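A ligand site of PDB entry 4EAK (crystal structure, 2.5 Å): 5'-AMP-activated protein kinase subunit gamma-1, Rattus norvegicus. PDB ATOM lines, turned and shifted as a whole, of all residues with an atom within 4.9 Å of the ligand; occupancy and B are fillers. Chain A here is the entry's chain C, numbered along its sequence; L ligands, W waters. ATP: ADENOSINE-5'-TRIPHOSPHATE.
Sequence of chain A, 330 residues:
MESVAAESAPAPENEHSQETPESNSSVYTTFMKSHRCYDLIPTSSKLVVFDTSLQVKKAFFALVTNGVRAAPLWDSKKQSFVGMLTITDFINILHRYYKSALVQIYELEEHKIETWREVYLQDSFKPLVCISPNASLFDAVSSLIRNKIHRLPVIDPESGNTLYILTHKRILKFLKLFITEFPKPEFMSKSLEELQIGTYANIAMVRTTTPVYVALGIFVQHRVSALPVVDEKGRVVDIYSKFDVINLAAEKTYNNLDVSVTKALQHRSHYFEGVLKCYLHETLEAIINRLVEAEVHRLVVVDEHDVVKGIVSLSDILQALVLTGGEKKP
O of Arg 151 sits at hydrogen-bond distance from N6 of the ligand (2.9 Å). NE of Arg 151 lies within salt-bridge range of O3G of the ligand. The side-chain carboxylate (OD2) of Asp 89 is in hydrogen-bond range of an oxygen (O3') of the ligand (2.5 Å). The backbone NH (N) of Thr 88 is in hydrogen-bond range of an oxygen (O2B) of the ligand, at 3.1 Å. The side-chain hydroxyl (OG1) of Thr 88 sits at hydrogen-bond distance from an oxygen (O2B) of the ligand, 2.7 Å away. The backbone NH (N) of Val 129 is in hydrogen-bond range of a nitrogen (N1) of the ligand (2.9 Å). A nitrogen (N6) of the ligand sits at hydrogen-bond distance from the backbone carbonyl oxygen of Val 129 (2.8 Å). The side-chain amide nitrogen (NE2) of Gln 122 sits at hydrogen-bond distance from an oxygen (O2') of the ligand. An oxygen (O2A) of the ligand lies within hydrogen-bond range of the backbone NH of His 150 (2.9 Å). A ring nitrogen (ND1) of His 150 is in hydrogen-bond range of an oxygen (O2G) of the ligand (3.1 Å). The side-chain hydroxyl (OG1) of Thr 86 sits at hydrogen-bond distance from an oxygen (O2B) of the ligand, at 2.9 Å. An oxygen (O2') of the ligand lies within hydrogen-bond range of the backbone carbonyl oxygen (O) of Met 84 (3.2 Å). An oxygen (O1G) of the ligand is in salt-bridge range of the guanidinium group (NH2) of Arg 69, 3.6 Å away.
The side-chain amide nitrogen of Gln 122 sits at hydrogen-bond distance from the side-chain carboxylate of Asp 89, at 3.2 Å. The side-chain carboxylate (OD1) of Asp 89 sits at hydrogen-bond distance from the backbone NH (N) of Thr 86. OG1 of Thr 88 sits at hydrogen-bond distance from NZ of Lys 242, 2.7 Å away. The backbone carbonyl oxygen of Thr 88 lies close to the side-chain amide oxygen of Asn 92 (3.4 Å). O of Arg 117 lies within hydrogen-bond range of N of Gln 122 (2.8 Å). NH1 of Arg 117 lies within hydrogen-bond range of O of Met 84 (3.3 Å).
Merely in contact with the ligand: Ile 87, Ile 149, Pro 153, Pro 127, Phe 243, Lys 126 and Leu 128. Hydrophobic or aromatic side chains within 4 Å of the ligand: Met 84, Ile 87, Val 129, Ile 149, His 150, Pro 153 and Phe 243. The nearest printed residue that does not touch the ligand is Lys 148 (4.1 Å).
Water W3 lies within hydrogen-bond range of an oxygen (O1G) of the ligand (2.6 Å), the backbone NH (N) of Ile 87 (2.7 Å) and the backbone carbonyl oxygen (O) of Arg 69 (2.9 Å). Water W4 lies within hydrogen-bond range of the backbone carbonyl oxygen (O) of Lys 126, the guanidinium group (NH2) of Arg 117 and a nitrogen (N3) of the ligand.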
ATOM      1  N   ARG A  69       1.336  10.558  19.465  1.00  0.00           N
ATOM      2  CA  ARG A  69       1.555   9.343  20.251  1.00  0.00           C
ATOM      3  C   ARG A  69       0.304   8.857  20.981  1.00  0.00           C
ATOM      4  O   ARG A  69       0.261   7.731  21.476  1.00  0.00           O
ATOM      5  CB  ARG A  69       2.722   9.544  21.234  1.00  0.00           C
ATOM      6  CG  ARG A  69       3.202  10.981  21.337  1.00  0.00           C
ATOM      7  CD  ARG A  69       4.658  11.065  21.812  1.00  0.00           C
ATOM      8  NE  ARG A  69       4.826  10.641  23.204  1.00  0.00           N
ATOM      9  CZ  ARG A  69       5.977  10.711  23.857  1.00  0.00           C
ATOM     10  NH1 ARG A  69       7.061  11.190  23.267  1.00  0.00           N
ATOM     11  NH2 ARG A  69       6.045  10.304  25.124  1.00  0.00           N
ATOM     12  N   GLY A  83     -11.795   7.671  27.220  1.00  0.00           N
ATOM     13  CA  GLY A  83     -10.404   7.616  27.643  1.00  0.00           C
ATOM     14  C   GLY A  83      -9.403   7.897  26.523  1.00  0.00           C
ATOM     15  O   GLY A  83      -9.753   8.447  25.491  1.00  0.00           O
ATOM     16  N   MET A  84      -8.159   7.501  26.768  1.00  0.00           N
ATOM     17  CA  MET A  84      -7.084   7.735  25.799  1.00  0.00           C
ATOM     18  C   MET A  84      -6.514   6.435  25.259  1.00  0.00           C
ATOM     19  O   MET A  84      -6.591   5.391  25.911  1.00  0.00           O
ATOM     20  CB  MET A  84      -5.955   8.554  26.458  1.00  0.00           C
ATOM     21  CG  MET A  84      -6.369   9.935  26.919  1.00  0.00           C
ATOM     22  SD  MET A  84      -6.771  11.041  25.555  1.00  0.00           S
ATOM     23  CE  MET A  84      -5.193  11.095  24.696  1.00  0.00           C
ATOM     24  N   THR A  86      -2.957   5.097  24.362  1.00  0.00           N
ATOM     25  CA  THR A  86      -1.556   5.437  24.510  1.00  0.00           C
ATOM     26  C   THR A  86      -0.633   4.241  24.263  1.00  0.00           C
ATOM     27  O   THR A  86      -1.092   3.115  24.097  1.00  0.00           O
ATOM     28  CB  THR A  86      -1.258   6.007  25.912  1.00  0.00           C
ATOM     29  OG1 THR A  86      -1.468   4.995  26.898  1.00  0.00           O
ATOM     30  CG2 THR A  86      -2.159   7.200  26.192  1.00  0.00           C
ATOM     31  N   ILE A  87       0.661   4.516  24.249  1.00  0.00           N
ATOM     32  CA  ILE A  87       1.677   3.496  24.026  1.00  0.00           C
ATOM     33  C   ILE A  87       1.552   2.364  25.045  1.00  0.00           C
ATOM     34  O   ILE A  87       1.795   1.200  24.719  1.00  0.00           O
ATOM     35  CB  ILE A  87       3.094   4.103  24.099  1.00  0.00           C
ATOM     36  CG1 ILE A  87       4.142   3.115  23.574  1.00  0.00           C
ATOM     37  CG2 ILE A  87       3.421   4.564  25.522  1.00  0.00           C
ATOM     38  CD1 ILE A  87       4.148   2.990  22.071  1.00  0.00           C
ATOM     39  N   THR A  88       1.163   2.711  26.260  1.00  0.00           N
ATOM     40  CA  THR A  88       0.994   1.721  27.329  1.00  0.00           C
ATOM     41  C   THR A  88      -0.082   0.702  26.990  1.00  0.00           C
ATOM     42  O   THR A  88       0.072  -0.485  27.250  1.00  0.00           O
ATOM     43  CB  THR A  88       0.658   2.397  28.674  1.00  0.00           C
ATOM     44  OG1 THR A  88       1.797   3.117  29.155  1.00  0.00           O
ATOM     45  CG2 THR A  88       0.260   1.357  29.706  1.00  0.00           C
ATOM     46  N   ASP A  89      -1.173   1.191  26.408  1.00  0.00           N
ATOM     47  CA  ASP A  89      -2.255   0.311  25.975  1.00  0.00           C
ATOM     48  C   ASP A  89      -1.749  -0.724  24.983  1.00  0.00           C
ATOM     49  O   ASP A  89      -2.128  -1.894  25.036  1.00  0.00           O
ATOM     50  CB  ASP A  89      -3.401   1.121  25.367  1.00  0.00           C
ATOM     51  CG  ASP A  89      -4.136   1.944  26.405  1.00  0.00           C
ATOM     52  OD1 ASP A  89      -4.484   3.111  26.112  1.00  0.00           O
ATOM     53  OD2 ASP A  89      -4.380   1.433  27.518  1.00  0.00           O
ATOM     54  N   ASN A  92       0.486  -3.250  26.957  1.00  0.00           N
ATOM     55  CA  ASN A  92      -0.368  -4.248  27.592  1.00  0.00           C
ATOM     56  C   ASN A  92      -0.870  -5.268  26.584  1.00  0.00           C
ATOM     57  O   ASN A  92      -0.772  -6.482  26.807  1.00  0.00           O
ATOM     58  CB  ASN A  92      -1.536  -3.580  28.301  1.00  0.00           C
ATOM     59  CG  ASN A  92      -1.090  -2.608  29.387  1.00  0.00           C
ATOM     60  OD1 ASN A  92       0.038  -2.686  29.879  1.00  0.00           O
ATOM     61  ND2 ASN A  92      -1.972  -1.684  29.756  1.00  0.00           N
ATOM     62  N   ARG A 117     -10.160  -2.786  25.318  1.00  0.00           N
ATOM     63  CA  ARG A 117     -10.468  -2.051  26.531  1.00  0.00           C
ATOM     64  C   ARG A 117     -11.387  -2.851  27.434  1.00  0.00           C
ATOM     65  O   ARG A 117     -11.290  -2.776  28.656  1.00  0.00           O
ATOM     66  CB  ARG A 117     -11.088  -0.678  26.210  1.00  0.00           C
ATOM     67  CG  ARG A 117     -10.124   0.297  25.540  1.00  0.00           C
ATOM     68  CD  ARG A 117     -10.778   1.665  25.333  1.00  0.00           C
ATOM     69  NE  ARG A 117     -11.104   2.308  26.600  1.00  0.00           N
ATOM     70  CZ  ARG A 117     -10.267   3.094  27.274  1.00  0.00           C
ATOM     71  NH1 ARG A 117      -9.046   3.326  26.806  1.00  0.00           N
ATOM     72  NH2 ARG A 117     -10.645   3.646  28.425  1.00  0.00           N
ATOM     73  N   GLN A 122     -11.460  -1.388  31.058  1.00  0.00           N
ATOM     74  CA  GLN A 122     -10.738  -0.127  31.257  1.00  0.00           C
ATOM     75  C   GLN A 122     -11.654   1.044  31.616  1.00  0.00           C
ATOM     76  O   GLN A 122     -11.331   1.837  32.497  1.00  0.00           O
ATOM     77  CB  GLN A 122      -9.903   0.200  30.009  1.00  0.00           C
ATOM     78  CG  GLN A 122      -8.890   1.308  30.216  1.00  0.00           C
ATOM     79  CD  GLN A 122      -7.832   1.334  29.126  1.00  0.00           C
ATOM     80  OE1 GLN A 122      -7.832   0.493  28.229  1.00  0.00           O
ATOM     81  NE2 GLN A 122      -6.928   2.296  29.202  1.00  0.00           N
ATOM     82  N   LYS A 126     -10.270   2.221  35.145  1.00  0.00           N
ATOM     83  CA  LYS A 126      -9.528   3.469  34.964  1.00  0.00           C
ATOM     84  C   LYS A 126     -10.335   4.404  34.091  1.00  0.00           C
ATOM     85  O   LYS A 126     -10.043   4.586  32.902  1.00  0.00           O
ATOM     86  CB  LYS A 126      -8.163   3.221  34.337  1.00  0.00           C
ATOM     87  CG  LYS A 126      -6.999   3.854  35.091  1.00  0.00           C
ATOM     88  CD  LYS A 126      -6.672   5.218  34.529  1.00  0.00           C
ATOM     89  CE  LYS A 126      -7.262   6.328  35.389  1.00  0.00           C
ATOM     90  NZ  LYS A 126      -6.428   6.485  36.615  1.00  0.00           N
ATOM     91  N   PRO A 127     -11.373   5.021  34.679  1.00  0.00           N
ATOM     92  CA  PRO A 127     -12.328   5.794  33.888  1.00  0.00           C
ATOM     93  C   PRO A 127     -11.701   7.046  33.331  1.00  0.00           C
ATOM     94  O   PRO A 127     -10.689   7.498  33.861  1.00  0.00           O
ATOM     95  CB  PRO A 127     -13.398   6.175  34.919  1.00  0.00           C
ATOM     96  CG  PRO A 127     -13.182   5.249  36.105  1.00  0.00           C
ATOM     97  CD  PRO A 127     -11.715   4.980  36.110  1.00  0.00           C
ATOM     98  N   LEU A 128     -12.288   7.622  32.283  1.00  0.00           N
ATOM     99  CA  LEU A 128     -11.718   8.840  31.712  1.00  0.00           C
ATOM    100  C   LEU A 128     -11.455   9.927  32.744  1.00  0.00           C
ATOM    101  O   LEU A 128     -12.348  10.262  33.518  1.00  0.00           O
ATOM    102  CB  LEU A 128     -12.609   9.440  30.609  1.00  0.00           C
ATOM    103  CG  LEU A 128     -12.280  10.879  30.144  1.00  0.00           C
ATOM    104  CD1 LEU A 128     -11.022  10.885  29.330  1.00  0.00           C
ATOM    105  CD2 LEU A 128     -13.410  11.509  29.359  1.00  0.00           C
ATOM    106  N   VAL A 129     -10.252  10.491  32.736  1.00  0.00           N
ATOM    107  CA  VAL A 129      -9.957  11.683  33.542  1.00  0.00           C
ATOM    108  C   VAL A 129      -9.821  12.869  32.590  1.00  0.00           C
ATOM    109  O   VAL A 129      -8.965  12.864  31.708  1.00  0.00           O
ATOM    110  CB  VAL A 129      -8.650  11.535  34.343  1.00  0.00           C
ATOM    111  CG1 VAL A 129      -8.406  12.780  35.185  1.00  0.00           C
ATOM    112  CG2 VAL A 129      -8.683  10.295  35.214  1.00  0.00           C
ATOM    113  N   LYS A 148      -1.820   9.410  38.033  1.00  0.00           N
ATOM    114  CA  LYS A 148      -0.727   8.710  37.380  1.00  0.00           C
ATOM    115  C   LYS A 148      -0.932   8.545  35.877  1.00  0.00           C
ATOM    116  O   LYS A 148      -0.741   7.466  35.317  1.00  0.00           O
ATOM    117  CB  LYS A 148      -0.496   7.340  38.041  1.00  0.00           C
ATOM    118  CG  LYS A 148       0.121   7.418  39.434  1.00  0.00           C
ATOM    119  CD  LYS A 148      -0.365   6.298  40.326  1.00  0.00           C
ATOM    120  CE  LYS A 148       0.288   6.332  41.693  1.00  0.00           C
ATOM    121  NZ  LYS A 148       1.711   5.892  41.643  1.00  0.00           N
ATOM    122  N   ILE A 149      -1.324   9.632  35.227  1.00  0.00           N
ATOM    123  CA  ILE A 149      -1.494   9.652  33.773  1.00  0.00           C
ATOM    124  C   ILE A 149      -0.705  10.812  33.178  1.00  0.00           C
ATOM    125  O   ILE A 149      -0.369  11.771  33.872  1.00  0.00           O
ATOM    126  CB  ILE A 149      -2.971   9.784  33.374  1.00  0.00           C
ATOM    127  CG1 ILE A 149      -3.614  10.985  34.073  1.00  0.00           C
ATOM    128  CG2 ILE A 149      -3.730   8.508  33.694  1.00  0.00           C
ATOM    129  CD1 ILE A 149      -5.039  11.265  33.639  1.00  0.00           C
ATOM    130  N   HIS A 150      -0.405  10.721  31.883  1.00  0.00           N
ATOM    131  CA  HIS A 150       0.373  11.756  31.203  1.00  0.00           C
ATOM    132  C   HIS A 150      -0.471  12.602  30.253  1.00  0.00           C
ATOM    133  O   HIS A 150      -0.031  13.670  29.800  1.00  0.00           O
ATOM    134  CB  HIS A 150       1.550  11.143  30.457  1.00  0.00           C
ATOM    135  CG  HIS A 150       2.515  10.418  31.340  1.00  0.00           C
ATOM    136  ND1 HIS A 150       3.054   9.188  31.012  1.00  0.00           N
ATOM    137  CD2 HIS A 150       3.039  10.733  32.546  1.00  0.00           C
ATOM    138  CE1 HIS A 150       3.870   8.791  31.963  1.00  0.00           C
ATOM    139  NE2 HIS A 150       3.876   9.710  32.920  1.00  0.00           N
ATOM    140  N   ARG A 151      -1.674  12.139  29.949  1.00  0.00           N
ATOM    141  CA  ARG A 151      -2.577  12.858  29.063  1.00  0.00           C
ATOM    142  C   ARG A 151      -3.814  13.320  29.813  1.00  0.00           C
ATOM    143  O   ARG A 151      -4.439  12.552  30.545  1.00  0.00           O
ATOM    144  CB  ARG A 151      -2.993  11.966  27.891  1.00  0.00           C
ATOM    145  CG  ARG A 151      -1.832  11.318  27.153  1.00  0.00           C
ATOM    146  CD  ARG A 151      -1.102  12.289  26.239  1.00  0.00           C
ATOM    147  NE  ARG A 151       0.053  11.654  25.600  1.00  0.00           N
ATOM    148  CZ  ARG A 151       0.857  12.244  24.732  1.00  0.00           C
ATOM    149  NH1 ARG A 151       0.649  13.500  24.368  1.00  0.00           N
ATOM    150  NH2 ARG A 151       1.878  11.571  24.209  1.00  0.00           N
ATOM    151  N   LEU A 152      -4.179  14.594  29.620  1.00  0.00           N
ATOM    152  CA  LEU A 152      -5.367  15.145  30.263  1.00  0.00           C
ATOM    153  C   LEU A 152      -6.200  15.940  29.255  1.00  0.00           C
ATOM    154  O   LEU A 152      -5.915  17.110  29.001  1.00  0.00           O
ATOM    155  CB  LEU A 152      -4.987  16.034  31.445  1.00  0.00           C
ATOM    156  CG  LEU A 152      -6.133  16.476  32.349  1.00  0.00           C
ATOM    157  CD1 LEU A 152      -6.859  15.262  32.924  1.00  0.00           C
ATOM    158  CD2 LEU A 152      -5.624  17.373  33.474  1.00  0.00           C
ATOM    159  N   PRO A 153      -7.218  15.303  28.680  1.00  0.00           N
ATOM    160  CA  PRO A 153      -8.103  15.949  27.707  1.00  0.00           C
ATOM    161  C   PRO A 153      -8.794  17.170  28.296  1.00  0.00           C
ATOM    162  O   PRO A 153      -9.395  17.079  29.365  1.00  0.00           O
ATOM    163  CB  PRO A 153      -9.136  14.870  27.384  1.00  0.00           C
ATOM    164  CG  PRO A 153      -8.465  13.580  27.727  1.00  0.00           C
ATOM    165  CD  PRO A 153      -7.591  13.886  28.902  1.00  0.00           C
ATOM    166  N   LYS A 242       9.220   2.259  26.167  1.00  0.00           N
ATOM    167  CA  LYS A 242       8.073   1.504  25.666  1.00  0.00           C
ATOM    168  C   LYS A 242       7.972   1.615  24.152  1.00  0.00           C
ATOM    169  O   LYS A 242       7.540   0.671  23.484  1.00  0.00           O
ATOM    170  CB  LYS A 242       6.787   2.013  26.320  1.00  0.00           C
ATOM    171  CG  LYS A 242       6.670   1.703  27.805  1.00  0.00           C
ATOM    172  CD  LYS A 242       5.393   2.273  28.398  1.00  0.00           C
ATOM    173  CE  LYS A 242       5.199   1.807  29.826  1.00  0.00           C
ATOM    174  NZ  LYS A 242       4.016   2.434  30.470  1.00  0.00           N
ATOM    175  N   PHE A 243       8.351   2.770  23.613  1.00  0.00           N
ATOM    176  CA  PHE A 243       8.284   3.005  22.180  1.00  0.00           C
ATOM    177  C   PHE A 243       9.268   2.130  21.419  1.00  0.00           C
ATOM    178  O   PHE A 243       8.986   1.683  20.312  1.00  0.00           O
ATOM    179  CB  PHE A 243       8.531   4.483  21.877  1.00  0.00           C
ATOM    180  CG  PHE A 243       7.519   5.407  22.493  1.00  0.00           C
ATOM    181  CD1 PHE A 243       7.768   5.996  23.725  1.00  0.00           C
ATOM    182  CD2 PHE A 243       6.328   5.682  21.852  1.00  0.00           C
ATOM    183  CE1 PHE A 243       6.832   6.844  24.300  1.00  0.00           C
ATOM    184  CE2 PHE A 243       5.392   6.530  22.427  1.00  0.00           C
ATOM    185  CZ  PHE A 243       5.656   7.111  23.650  1.00  0.00           C
HETATM  186  PG  ATP L   1       2.517   8.858  26.854  1.00  0.00           P
HETATM  187  O1G ATP L   1       3.033   8.434  25.554  1.00  0.00           O
HETATM  188  O2G ATP L   1       3.481   8.870  27.941  1.00  0.00           O
HETATM  189  O3G ATP L   1       1.661  10.043  26.727  1.00  0.00           O
HETATM  190  PB  ATP L   1       1.969   6.589  28.252  1.00  0.00           P
HETATM  191  O1B ATP L   1       3.412   6.586  28.504  1.00  0.00           O
HETATM  192  O2B ATP L   1       1.291   5.384  27.828  1.00  0.00           O
HETATM  193  O3B ATP L   1       1.545   7.734  27.283  1.00  0.00           O
HETATM  194  PA  ATP L   1      -0.205   7.469  29.916  1.00  0.00           P
HETATM  195  O1A ATP L   1      -0.669   8.422  28.959  1.00  0.00           O
HETATM  196  O2A ATP L   1      -0.183   7.901  31.292  1.00  0.00           O
HETATM  197  O3A ATP L   1       1.283   7.032  29.601  1.00  0.00           O
HETATM  198  O5' ATP L   1      -0.988   6.130  29.797  1.00  0.00           O
HETATM  199  C5' ATP L   1      -1.128   5.203  30.852  1.00  0.00           C
HETATM  200  C4' ATP L   1      -2.497   4.535  30.804  1.00  0.00           C
HETATM  201  O4' ATP L   1      -3.454   5.413  31.322  1.00  0.00           O
HETATM  202  C3' ATP L   1      -2.948   4.173  29.429  1.00  0.00           C
HETATM  203  O3' ATP L   1      -3.468   2.872  29.408  1.00  0.00           O
HETATM  204  C2' ATP L   1      -4.080   5.101  29.139  1.00  0.00           C
HETATM  205  O2' ATP L   1      -5.108   4.400  28.508  1.00  0.00           O
HETATM  206  C1' ATP L   1      -4.546   5.553  30.469  1.00  0.00           C
HETATM  207  N9  ATP L   1      -4.851   6.975  30.414  1.00  0.00           N
HETATM  208  C8  ATP L   1      -4.041   7.912  29.968  1.00  0.00           C
HETATM  209  N7  ATP L   1      -4.602   9.101  30.059  1.00  0.00           N
HETATM  210  C5  ATP L   1      -5.812   8.929  30.571  1.00  0.00           C
HETATM  211  C6  ATP L   1      -6.944   9.784  30.927  1.00  0.00           C
HETATM  212  N6  ATP L   1      -6.935  11.099  30.774  1.00  0.00           N
HETATM  213  N1  ATP L   1      -7.991   9.178  31.425  1.00  0.00           N
HETATM  214  C2  ATP L   1      -8.072   7.881  31.614  1.00  0.00           C
HETATM  215  N3  ATP L   1      -7.097   7.063  31.312  1.00  0.00           N
HETATM  216  C4  ATP L   1      -5.963   7.528  30.808  1.00  0.00           C
HETATM  217  O   HOH W   1      -7.632   5.450  28.676  1.00  0.00           O
HETATM  218  O   HOH W   2       5.788   6.977  27.817  1.00  0.00           O
HETATM  219  O   HOH W   3       1.256   7.105  24.180  1.00  0.00           O
HETATM  220  O   HOH W   4      -9.927   5.541  30.421  1.00  0.00           O
